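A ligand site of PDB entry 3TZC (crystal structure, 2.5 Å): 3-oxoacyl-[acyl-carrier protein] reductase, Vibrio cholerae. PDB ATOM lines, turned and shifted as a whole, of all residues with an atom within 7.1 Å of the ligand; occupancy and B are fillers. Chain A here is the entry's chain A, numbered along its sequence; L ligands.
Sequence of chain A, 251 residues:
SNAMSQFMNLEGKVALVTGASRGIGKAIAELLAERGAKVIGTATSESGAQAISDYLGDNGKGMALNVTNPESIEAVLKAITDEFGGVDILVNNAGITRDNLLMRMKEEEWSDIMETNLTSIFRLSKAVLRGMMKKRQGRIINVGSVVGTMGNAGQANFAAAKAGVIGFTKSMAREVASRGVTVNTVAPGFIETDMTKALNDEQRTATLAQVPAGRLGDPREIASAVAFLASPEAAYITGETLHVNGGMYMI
O of Gly 95 lies close to O1 of the ligand (3.5 Å). Ala 20 touches the ligand. Ala 43 touches the ligand (CB to O8, 2.8 Å). O of Leu 65 touches C9 of the ligand, at 3.3 Å. Ile 96 touches the ligand (CG2 to N2, 3.2 Å). Thr 116 touches the ligand.
The backbone NH (N) of Thr 44 sits at hydrogen-bond distance from an oxygen (O8) of the ligand (2.8 Å). OG1 of Thr 44 lies within hydrogen-bond range of O9 of the ligand (2.4 Å). The guanidinium group (NH2) of Arg 22 lies within salt-bridge range of an oxygen (O2) of the ligand (2.7 Å). OG of Ser 21 sits at hydrogen-bond distance from O10 of the ligand. The backbone carbonyl oxygen (O) of Gly 19 sits close to an oxygen (O5) of the ligand, 3.3 Å away. N of Val 67 lies within hydrogen-bond range of N4 of the ligand (3.1 Å). OG1 of Thr 97 sits at hydrogen-bond distance from O1 of the ligand (3.2 Å). The side-chain amide oxygen (OD1) of Asn 66 sits at hydrogen-bond distance from a nitrogen (N3) of the ligand.
The backbone carbonyl oxygen (O) of Ala 43 is in hydrogen-bond range of the backbone NH (N) of Leu 65. The backbone NH (N) of Gly 19 sits at hydrogen-bond distance from the backbone carbonyl oxygen (O) of Thr 42, at 3.2 Å. The backbone carbonyl oxygen (O) of Gly 19 sits at hydrogen-bond distance from the side-chain amide nitrogen (ND2) of Asn 93 (3.3 Å). OD1 of Asn 66 sits at hydrogen-bond distance from OG1 of Thr 68. The side-chain hydroxyl (OG1) of Thr 116 lies within hydrogen-bond range of the backbone carbonyl oxygen (O) of Asp 112 (2.6 Å). OG of Ser 120 lies within hydrogen-bond range of O of Thr 116 (2.6 Å). The backbone carbonyl oxygen (O) of Thr 42 lies within hydrogen-bond range of the backbone NH (N) of Ala 20 (2.9 Å).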
ATOM      1  N   THR A  18      11.123 -19.808 -11.154  1.00  0.00           N
ATOM      2  CA  THR A  18      11.676 -18.454 -11.276  1.00  0.00           C
ATOM      3  C   THR A  18      13.105 -18.501 -11.781  1.00  0.00           C
ATOM      4  O   THR A  18      13.823 -19.432 -11.484  1.00  0.00           O
ATOM      5  CB  THR A  18      11.686 -17.721  -9.922  1.00  0.00           C
ATOM      6  OG1 THR A  18      12.549 -18.416  -9.005  1.00  0.00           O
ATOM      7  CG2 THR A  18      10.303 -17.645  -9.318  1.00  0.00           C
ATOM      8  N   GLY A  19      13.510 -17.535 -12.600  1.00  0.00           N
ATOM      9  CA  GLY A  19      14.865 -17.494 -13.128  1.00  0.00           C
ATOM     10  C   GLY A  19      15.139 -18.621 -14.114  1.00  0.00           C
ATOM     11  O   GLY A  19      16.210 -19.233 -14.084  1.00  0.00           O
ATOM     12  N   ALA A  20      14.193 -18.822 -15.033  1.00  0.00           N
ATOM     13  CA  ALA A  20      14.190 -20.020 -15.890  1.00  0.00           C
ATOM     14  C   ALA A  20      14.800 -19.843 -17.262  1.00  0.00           C
ATOM     15  O   ALA A  20      14.623 -20.703 -18.124  1.00  0.00           O
ATOM     16  CB  ALA A  20      12.777 -20.574 -16.033  1.00  0.00           C
ATOM     17  N   SER A  21      15.511 -18.738 -17.493  1.00  0.00           N
ATOM     18  CA  SER A  21      15.930 -18.414 -18.852  1.00  0.00           C
ATOM     19  C   SER A  21      17.186 -19.182 -19.274  1.00  0.00           C
ATOM     20  O   SER A  21      17.412 -19.365 -20.462  1.00  0.00           O
ATOM     21  CB  SER A  21      16.107 -16.912 -19.048  1.00  0.00           C
ATOM     22  OG  SER A  21      17.182 -16.436 -18.283  1.00  0.00           O
ATOM     23  N   ARG A  22      17.981 -19.653 -18.318  1.00  0.00           N
ATOM     24  CA  ARG A  22      19.182 -20.407 -18.644  1.00  0.00           C
ATOM     25  C   ARG A  22      19.701 -21.270 -17.487  1.00  0.00           C
ATOM     26  O   ARG A  22      19.180 -21.219 -16.361  1.00  0.00           O
ATOM     27  CB  ARG A  22      20.305 -19.475 -19.137  1.00  0.00           C
ATOM     28  CG  ARG A  22      20.803 -18.484 -18.115  1.00  0.00           C
ATOM     29  CD  ARG A  22      22.065 -17.792 -18.606  1.00  0.00           C
ATOM     30  NE  ARG A  22      22.316 -16.558 -17.847  1.00  0.00           N
ATOM     31  CZ  ARG A  22      22.777 -16.533 -16.591  1.00  0.00           C
ATOM     32  NH1 ARG A  22      23.038 -17.660 -15.947  1.00  0.00           N
ATOM     33  NH2 ARG A  22      22.969 -15.360 -15.975  1.00  0.00           N
ATOM     34  N   GLY A  25      18.012 -23.009 -13.963  1.00  0.00           N
ATOM     35  CA  GLY A  25      16.593 -22.706 -14.056  1.00  0.00           C
ATOM     36  C   GLY A  25      15.919 -23.261 -15.283  1.00  0.00           C
ATOM     37  O   GLY A  25      14.801 -23.813 -15.217  1.00  0.00           O
ATOM     38  N   THR A  42      10.071 -17.821 -15.542  1.00  0.00           N
ATOM     39  CA  THR A  42      10.132 -16.385 -15.515  1.00  0.00           C
ATOM     40  C   THR A  42      11.537 -15.861 -15.805  1.00  0.00           C
ATOM     41  O   THR A  42      12.543 -16.524 -15.499  1.00  0.00           O
ATOM     42  CB  THR A  42       9.692 -15.819 -14.159  1.00  0.00           C
ATOM     43  OG1 THR A  42      10.708 -16.044 -13.183  1.00  0.00           O
ATOM     44  CG2 THR A  42       8.413 -16.461 -13.665  1.00  0.00           C
ATOM     45  N   ALA A  43      11.563 -14.669 -16.407  1.00  0.00           N
ATOM     46  CA  ALA A  43      12.759 -13.874 -16.567  1.00  0.00           C
ATOM     47  C   ALA A  43      12.435 -12.414 -16.186  1.00  0.00           C
ATOM     48  O   ALA A  43      11.279 -12.066 -15.948  1.00  0.00           O
ATOM     49  CB  ALA A  43      13.192 -13.925 -18.015  1.00  0.00           C
ATOM     50  N   THR A  44      13.452 -11.567 -16.133  1.00  0.00           N
ATOM     51  CA  THR A  44      13.250 -10.158 -15.801  1.00  0.00           C
ATOM     52  C   THR A  44      12.677  -9.354 -16.974  1.00  0.00           C
ATOM     53  O   THR A  44      12.010  -8.354 -16.742  1.00  0.00           O
ATOM     54  CB  THR A  44      14.547  -9.499 -15.267  1.00  0.00           C
ATOM     55  OG1 THR A  44      15.665  -9.954 -16.031  1.00  0.00           O
ATOM     56  CG2 THR A  44      14.728  -9.884 -13.794  1.00  0.00           C
ATOM     57  N   SER A  45      12.930  -9.769 -18.212  1.00  0.00           N
ATOM     58  CA  SER A  45      12.455  -9.034 -19.398  1.00  0.00           C
ATOM     59  C   SER A  45      11.452  -9.837 -20.211  1.00  0.00           C
ATOM     60  O   SER A  45      11.274 -11.031 -19.966  1.00  0.00           O
ATOM     61  CB  SER A  45      13.624  -8.607 -20.294  1.00  0.00           C
ATOM     62  OG  SER A  45      14.378  -9.728 -20.712  1.00  0.00           O
ATOM     63  N   SER A  47      11.684 -10.353 -23.492  1.00  0.00           N
ATOM     64  CA  SER A  47      12.461 -11.184 -24.423  1.00  0.00           C
ATOM     65  C   SER A  47      13.015 -12.435 -23.708  1.00  0.00           C
ATOM     66  O   SER A  47      13.296 -13.446 -24.331  1.00  0.00           O
ATOM     67  CB  SER A  47      13.601 -10.373 -25.024  1.00  0.00           C
ATOM     68  OG  SER A  47      14.496  -9.956 -24.010  1.00  0.00           O
ATOM     69  N   GLY A  48      13.184 -12.330 -22.392  1.00  0.00           N
ATOM     70  CA  GLY A  48      13.495 -13.484 -21.557  1.00  0.00           C
ATOM     71  C   GLY A  48      12.291 -14.397 -21.570  1.00  0.00           C
ATOM     72  O   GLY A  48      12.389 -15.552 -21.960  1.00  0.00           O
ATOM     73  N   ALA A  49      11.147 -13.828 -21.192  1.00  0.00           N
ATOM     74  CA  ALA A  49       9.867 -14.528 -21.184  1.00  0.00           C
ATOM     75  C   ALA A  49       9.588 -15.219 -22.519  1.00  0.00           C
ATOM     76  O   ALA A  49       9.202 -16.375 -22.554  1.00  0.00           O
ATOM     77  CB  ALA A  49       8.749 -13.559 -20.849  1.00  0.00           C
ATOM     78  N   ILE A  52      11.765 -18.283 -23.074  1.00  0.00           N
ATOM     79  CA  ILE A  52      11.222 -19.369 -22.258  1.00  0.00           C
ATOM     80  C   ILE A  52       9.968 -19.957 -22.927  1.00  0.00           C
ATOM     81  O   ILE A  52       9.801 -21.189 -22.964  1.00  0.00           O
ATOM     82  CB  ILE A  52      10.921 -18.888 -20.845  1.00  0.00           C
ATOM     83  CG1 ILE A  52      12.241 -18.539 -20.126  1.00  0.00           C
ATOM     84  CG2 ILE A  52      10.137 -19.929 -20.060  1.00  0.00           C
ATOM     85  CD1 ILE A  52      12.132 -17.807 -18.843  1.00  0.00           C
ATOM     86  N   LEU A  65       8.731 -11.377 -14.624  1.00  0.00           N
ATOM     87  CA  LEU A  65       8.503 -11.277 -13.188  1.00  0.00           C
ATOM     88  C   LEU A  65       9.724 -10.627 -12.531  1.00  0.00           C
ATOM     89  O   LEU A  65      10.870 -10.984 -12.819  1.00  0.00           O
ATOM     90  CB  LEU A  65       8.270 -12.661 -12.591  1.00  0.00           C
ATOM     91  CG  LEU A  65       8.061 -12.779 -11.062  1.00  0.00           C
ATOM     92  CD1 LEU A  65       6.858 -11.919 -10.624  1.00  0.00           C
ATOM     93  CD2 LEU A  65       7.898 -14.231 -10.607  1.00  0.00           C
ATOM     94  N   ASN A  66       9.469  -9.632 -11.690  1.00  0.00           N
ATOM     95  CA  ASN A  66      10.493  -9.087 -10.803  1.00  0.00           C
ATOM     96  C   ASN A  66      10.184  -9.594  -9.377  1.00  0.00           C
ATOM     97  O   ASN A  66       9.174  -9.223  -8.779  1.00  0.00           O
ATOM     98  CB  ASN A  66      10.499  -7.564 -10.850  1.00  0.00           C
ATOM     99  CG  ASN A  66      11.592  -6.947  -9.991  1.00  0.00           C
ATOM    100  OD1 ASN A  66      12.280  -7.650  -9.232  1.00  0.00           O
ATOM    101  ND2 ASN A  66      11.773  -5.626 -10.098  1.00  0.00           N
ATOM    102  N   VAL A  67      11.026 -10.488  -8.883  1.00  0.00           N
ATOM    103  CA  VAL A  67      10.778 -11.153  -7.592  1.00  0.00           C
ATOM    104  C   VAL A  67      10.827 -10.193  -6.402  1.00  0.00           C
ATOM    105  O   VAL A  67      10.209 -10.448  -5.374  1.00  0.00           O
ATOM    106  CB  VAL A  67      11.742 -12.338  -7.384  1.00  0.00           C
ATOM    107  CG1 VAL A  67      11.305 -13.536  -8.230  1.00  0.00           C
ATOM    108  CG2 VAL A  67      13.180 -11.930  -7.624  1.00  0.00           C
ATOM    109  N   THR A  68      11.510  -9.061  -6.559  1.00  0.00           N
ATOM    110  CA  THR A  68      11.556  -8.048  -5.503  1.00  0.00           C
ATOM    111  C   THR A  68      10.306  -7.159  -5.414  1.00  0.00           C
ATOM    112  O   THR A  68      10.197  -6.354  -4.501  1.00  0.00           O
ATOM    113  CB  THR A  68      12.778  -7.147  -5.674  1.00  0.00           C
ATOM    114  OG1 THR A  68      12.686  -6.452  -6.935  1.00  0.00           O
ATOM    115  CG2 THR A  68      14.062  -7.968  -5.635  1.00  0.00           C
ATOM    116  N   ASN A  69       9.338  -7.300  -6.332  1.00  0.00           N
ATOM    117  CA  ASN A  69       8.187  -6.381  -6.425  1.00  0.00           C
ATOM    118  C   ASN A  69       6.841  -7.075  -6.171  1.00  0.00           C
ATOM    119  O   ASN A  69       6.397  -7.867  -7.001  1.00  0.00           O
ATOM    120  CB  ASN A  69       8.186  -5.714  -7.797  1.00  0.00           C
ATOM    121  CG  ASN A  69       7.136  -4.638  -7.934  1.00  0.00           C
ATOM    122  OD1 ASN A  69       6.262  -4.469  -7.092  1.00  0.00           O
ATOM    123  ND2 ASN A  69       7.221  -3.912  -9.035  1.00  0.00           N
ATOM    124  N   ASN A  93      14.194 -20.184  -7.720  1.00  0.00           N
ATOM    125  CA  ASN A  93      15.529 -20.295  -8.242  1.00  0.00           C
ATOM    126  C   ASN A  93      16.116 -18.947  -8.581  1.00  0.00           C
ATOM    127  O   ASN A  93      17.317 -18.813  -8.708  1.00  0.00           O
ATOM    128  CB  ASN A  93      15.498 -21.248  -9.433  1.00  0.00           C
ATOM    129  CG  ASN A  93      16.840 -21.395 -10.101  1.00  0.00           C
ATOM    130  OD1 ASN A  93      17.774 -21.882  -9.500  1.00  0.00           O
ATOM    131  ND2 ASN A  93      16.922 -21.008 -11.367  1.00  0.00           N
ATOM    132  N   ALA A  94      15.279 -17.929  -8.694  1.00  0.00           N
ATOM    133  CA  ALA A  94      15.760 -16.570  -8.950  1.00  0.00           C
ATOM    134  C   ALA A  94      16.817 -16.189  -7.923  1.00  0.00           C
ATOM    135  O   ALA A  94      16.695 -16.503  -6.726  1.00  0.00           O
ATOM    136  CB  ALA A  94      14.609 -15.608  -8.919  1.00  0.00           C
ATOM    137  N   GLY A  95      17.889 -15.564  -8.438  1.00  0.00           N
ATOM    138  CA  GLY A  95      18.989 -15.093  -7.616  1.00  0.00           C
ATOM    139  C   GLY A  95      20.036 -14.377  -8.456  1.00  0.00           C
ATOM    140  O   GLY A  95      20.397 -14.868  -9.547  1.00  0.00           O
ATOM    141  N   ILE A  96      20.506 -13.225  -7.972  1.00  0.00           N
ATOM    142  CA  ILE A  96      21.608 -12.524  -8.624  1.00  0.00           C
ATOM    143  C   ILE A  96      22.909 -12.927  -7.950  1.00  0.00           C
ATOM    144  O   ILE A  96      23.202 -12.511  -6.842  1.00  0.00           O
ATOM    145  CB  ILE A  96      21.420 -10.993  -8.667  1.00  0.00           C
ATOM    146  CG1 ILE A  96      21.170 -10.390  -7.278  1.00  0.00           C
ATOM    147  CG2 ILE A  96      20.253 -10.638  -9.590  1.00  0.00           C
ATOM    148  CD1 ILE A  96      20.802  -8.919  -7.303  1.00  0.00           C
ATOM    149  N   THR A  97      23.658 -13.796  -8.607  1.00  0.00           N
ATOM    150  CA  THR A  97      24.931 -14.262  -8.114  1.00  0.00           C
ATOM    151  C   THR A  97      26.019 -13.289  -8.581  1.00  0.00           C
ATOM    152  O   THR A  97      26.698 -13.557  -9.563  1.00  0.00           O
ATOM    153  CB  THR A  97      25.196 -15.692  -8.636  1.00  0.00           C
ATOM    154  OG1 THR A  97      25.201 -15.673 -10.073  1.00  0.00           O
ATOM    155  CG2 THR A  97      24.098 -16.662  -8.149  1.00  0.00           C
ATOM    156  N   ARG A  98      26.144 -12.157  -7.884  1.00  0.00           N
ATOM    157  CA  ARG A  98      27.132 -11.124  -8.198  1.00  0.00           C
ATOM    158  C   ARG A  98      28.056 -10.828  -7.017  1.00  0.00           C
ATOM    159  O   ARG A  98      28.603  -9.727  -6.890  1.00  0.00           O
ATOM    160  CB  ARG A  98      26.428  -9.834  -8.642  1.00  0.00           C
ATOM    161  N   ASP A 112      19.139  -4.728  -2.315  1.00  0.00           N
ATOM    162  CA  ASP A 112      18.688  -5.425  -3.513  1.00  0.00           C
ATOM    163  C   ASP A 112      19.140  -6.878  -3.593  1.00  0.00           C
ATOM    164  O   ASP A 112      18.378  -7.718  -4.061  1.00  0.00           O
ATOM    165  CB  ASP A 112      19.203  -4.735  -4.793  1.00  0.00           C
ATOM    166  CG  ASP A 112      18.391  -3.522  -5.177  1.00  0.00           C
ATOM    167  OD1 ASP A 112      17.387  -3.217  -4.483  1.00  0.00           O
ATOM    168  OD2 ASP A 112      18.758  -2.860  -6.185  1.00  0.00           O
ATOM    169  N   THR A 116      16.272  -9.788  -3.524  1.00  0.00           N
ATOM    170  CA  THR A 116      16.234 -10.683  -4.671  1.00  0.00           C
ATOM    171  C   THR A 116      16.557 -12.132  -4.277  1.00  0.00           C
ATOM    172  O   THR A 116      15.881 -13.063  -4.741  1.00  0.00           O
ATOM    173  CB  THR A 116      17.198 -10.214  -5.774  1.00  0.00           C
ATOM    174  OG1 THR A 116      17.002  -8.832  -5.980  1.00  0.00           O
ATOM    175  CG2 THR A 116      16.949 -10.932  -7.119  1.00  0.00           C
ATOM    176  N   SER A 120      12.433 -12.573  -1.575  1.00  0.00           N
ATOM    177  CA  SER A 120      11.598 -13.019  -2.670  1.00  0.00           C
ATOM    178  C   SER A 120      11.068 -14.416  -2.406  1.00  0.00           C
ATOM    179  O   SER A 120       9.879 -14.685  -2.614  1.00  0.00           O
ATOM    180  CB  SER A 120      12.409 -13.009  -3.963  1.00  0.00           C
ATOM    181  OG  SER A 120      13.570 -13.804  -3.846  1.00  0.00           O
HETATM  182  P1  LIG L   1      22.102 -13.958 -12.919  1.00  0.00           P
HETATM  183  O1  LIG L   1      22.821 -14.933 -12.007  1.00  0.00           O
HETATM  184  O2  LIG L   1      22.873 -13.406 -14.094  1.00  0.00           O
HETATM  185  O3  LIG L   1      20.675 -14.575 -13.422  1.00  0.00           O
HETATM  186  C1  LIG L   1      20.097 -15.822 -12.999  1.00  0.00           C
HETATM  187  C2  LIG L   1      18.563 -15.826 -13.106  1.00  0.00           C
HETATM  188  O4  LIG L   1      17.965 -14.979 -12.095  1.00  0.00           O
HETATM  189  C3  LIG L   1      18.023 -15.311 -14.437  1.00  0.00           C
HETATM  190  O5  LIG L   1      16.974 -16.180 -14.906  1.00  0.00           O
HETATM  191  C4  LIG L   1      17.483 -13.911 -14.125  1.00  0.00           C
HETATM  192  O6  LIG L   1      16.478 -13.475 -15.052  1.00  0.00           O
HETATM  193  C5  LIG L   1      16.989 -14.077 -12.685  1.00  0.00           C
HETATM  194  N1  LIG L   1      16.855 -12.777 -11.934  1.00  0.00           N
HETATM  195  C6  LIG L   1      17.864 -11.962 -11.608  1.00  0.00           C
HETATM  196  N2  LIG L   1      17.403 -10.889 -10.933  1.00  0.00           N
HETATM  197  C7  LIG L   1      16.078 -10.976 -10.831  1.00  0.00           C
HETATM  198  C8  LIG L   1      15.007 -10.138 -10.239  1.00  0.00           C
HETATM  199  N3  LIG L   1      15.340  -8.972  -9.632  1.00  0.00           N
HETATM  200  N4  LIG L   1      13.727 -10.581 -10.335  1.00  0.00           N
HETATM  201  C9  LIG L   1      13.443 -11.766 -10.953  1.00  0.00           C
HETATM  202  N5  LIG L   1      14.394 -12.564 -11.524  1.00  0.00           N
HETATM  203  C10 LIG L   1      15.708 -12.223 -11.499  1.00  0.00           C
HETATM  204  O7  LIG L   1      21.620 -12.685 -12.067  1.00  0.00           O
HETATM  205  P2  LIG L   1      16.924 -12.879 -16.497  1.00  0.00           P
HETATM  206  O8  LIG L   1      15.683 -12.844 -17.354  1.00  0.00           O
HETATM  207  O9  LIG L   1      17.494 -11.546 -16.148  1.00  0.00           O
HETATM  208  O10 LIG L   1      17.954 -13.858 -16.993  1.00  0.00           O
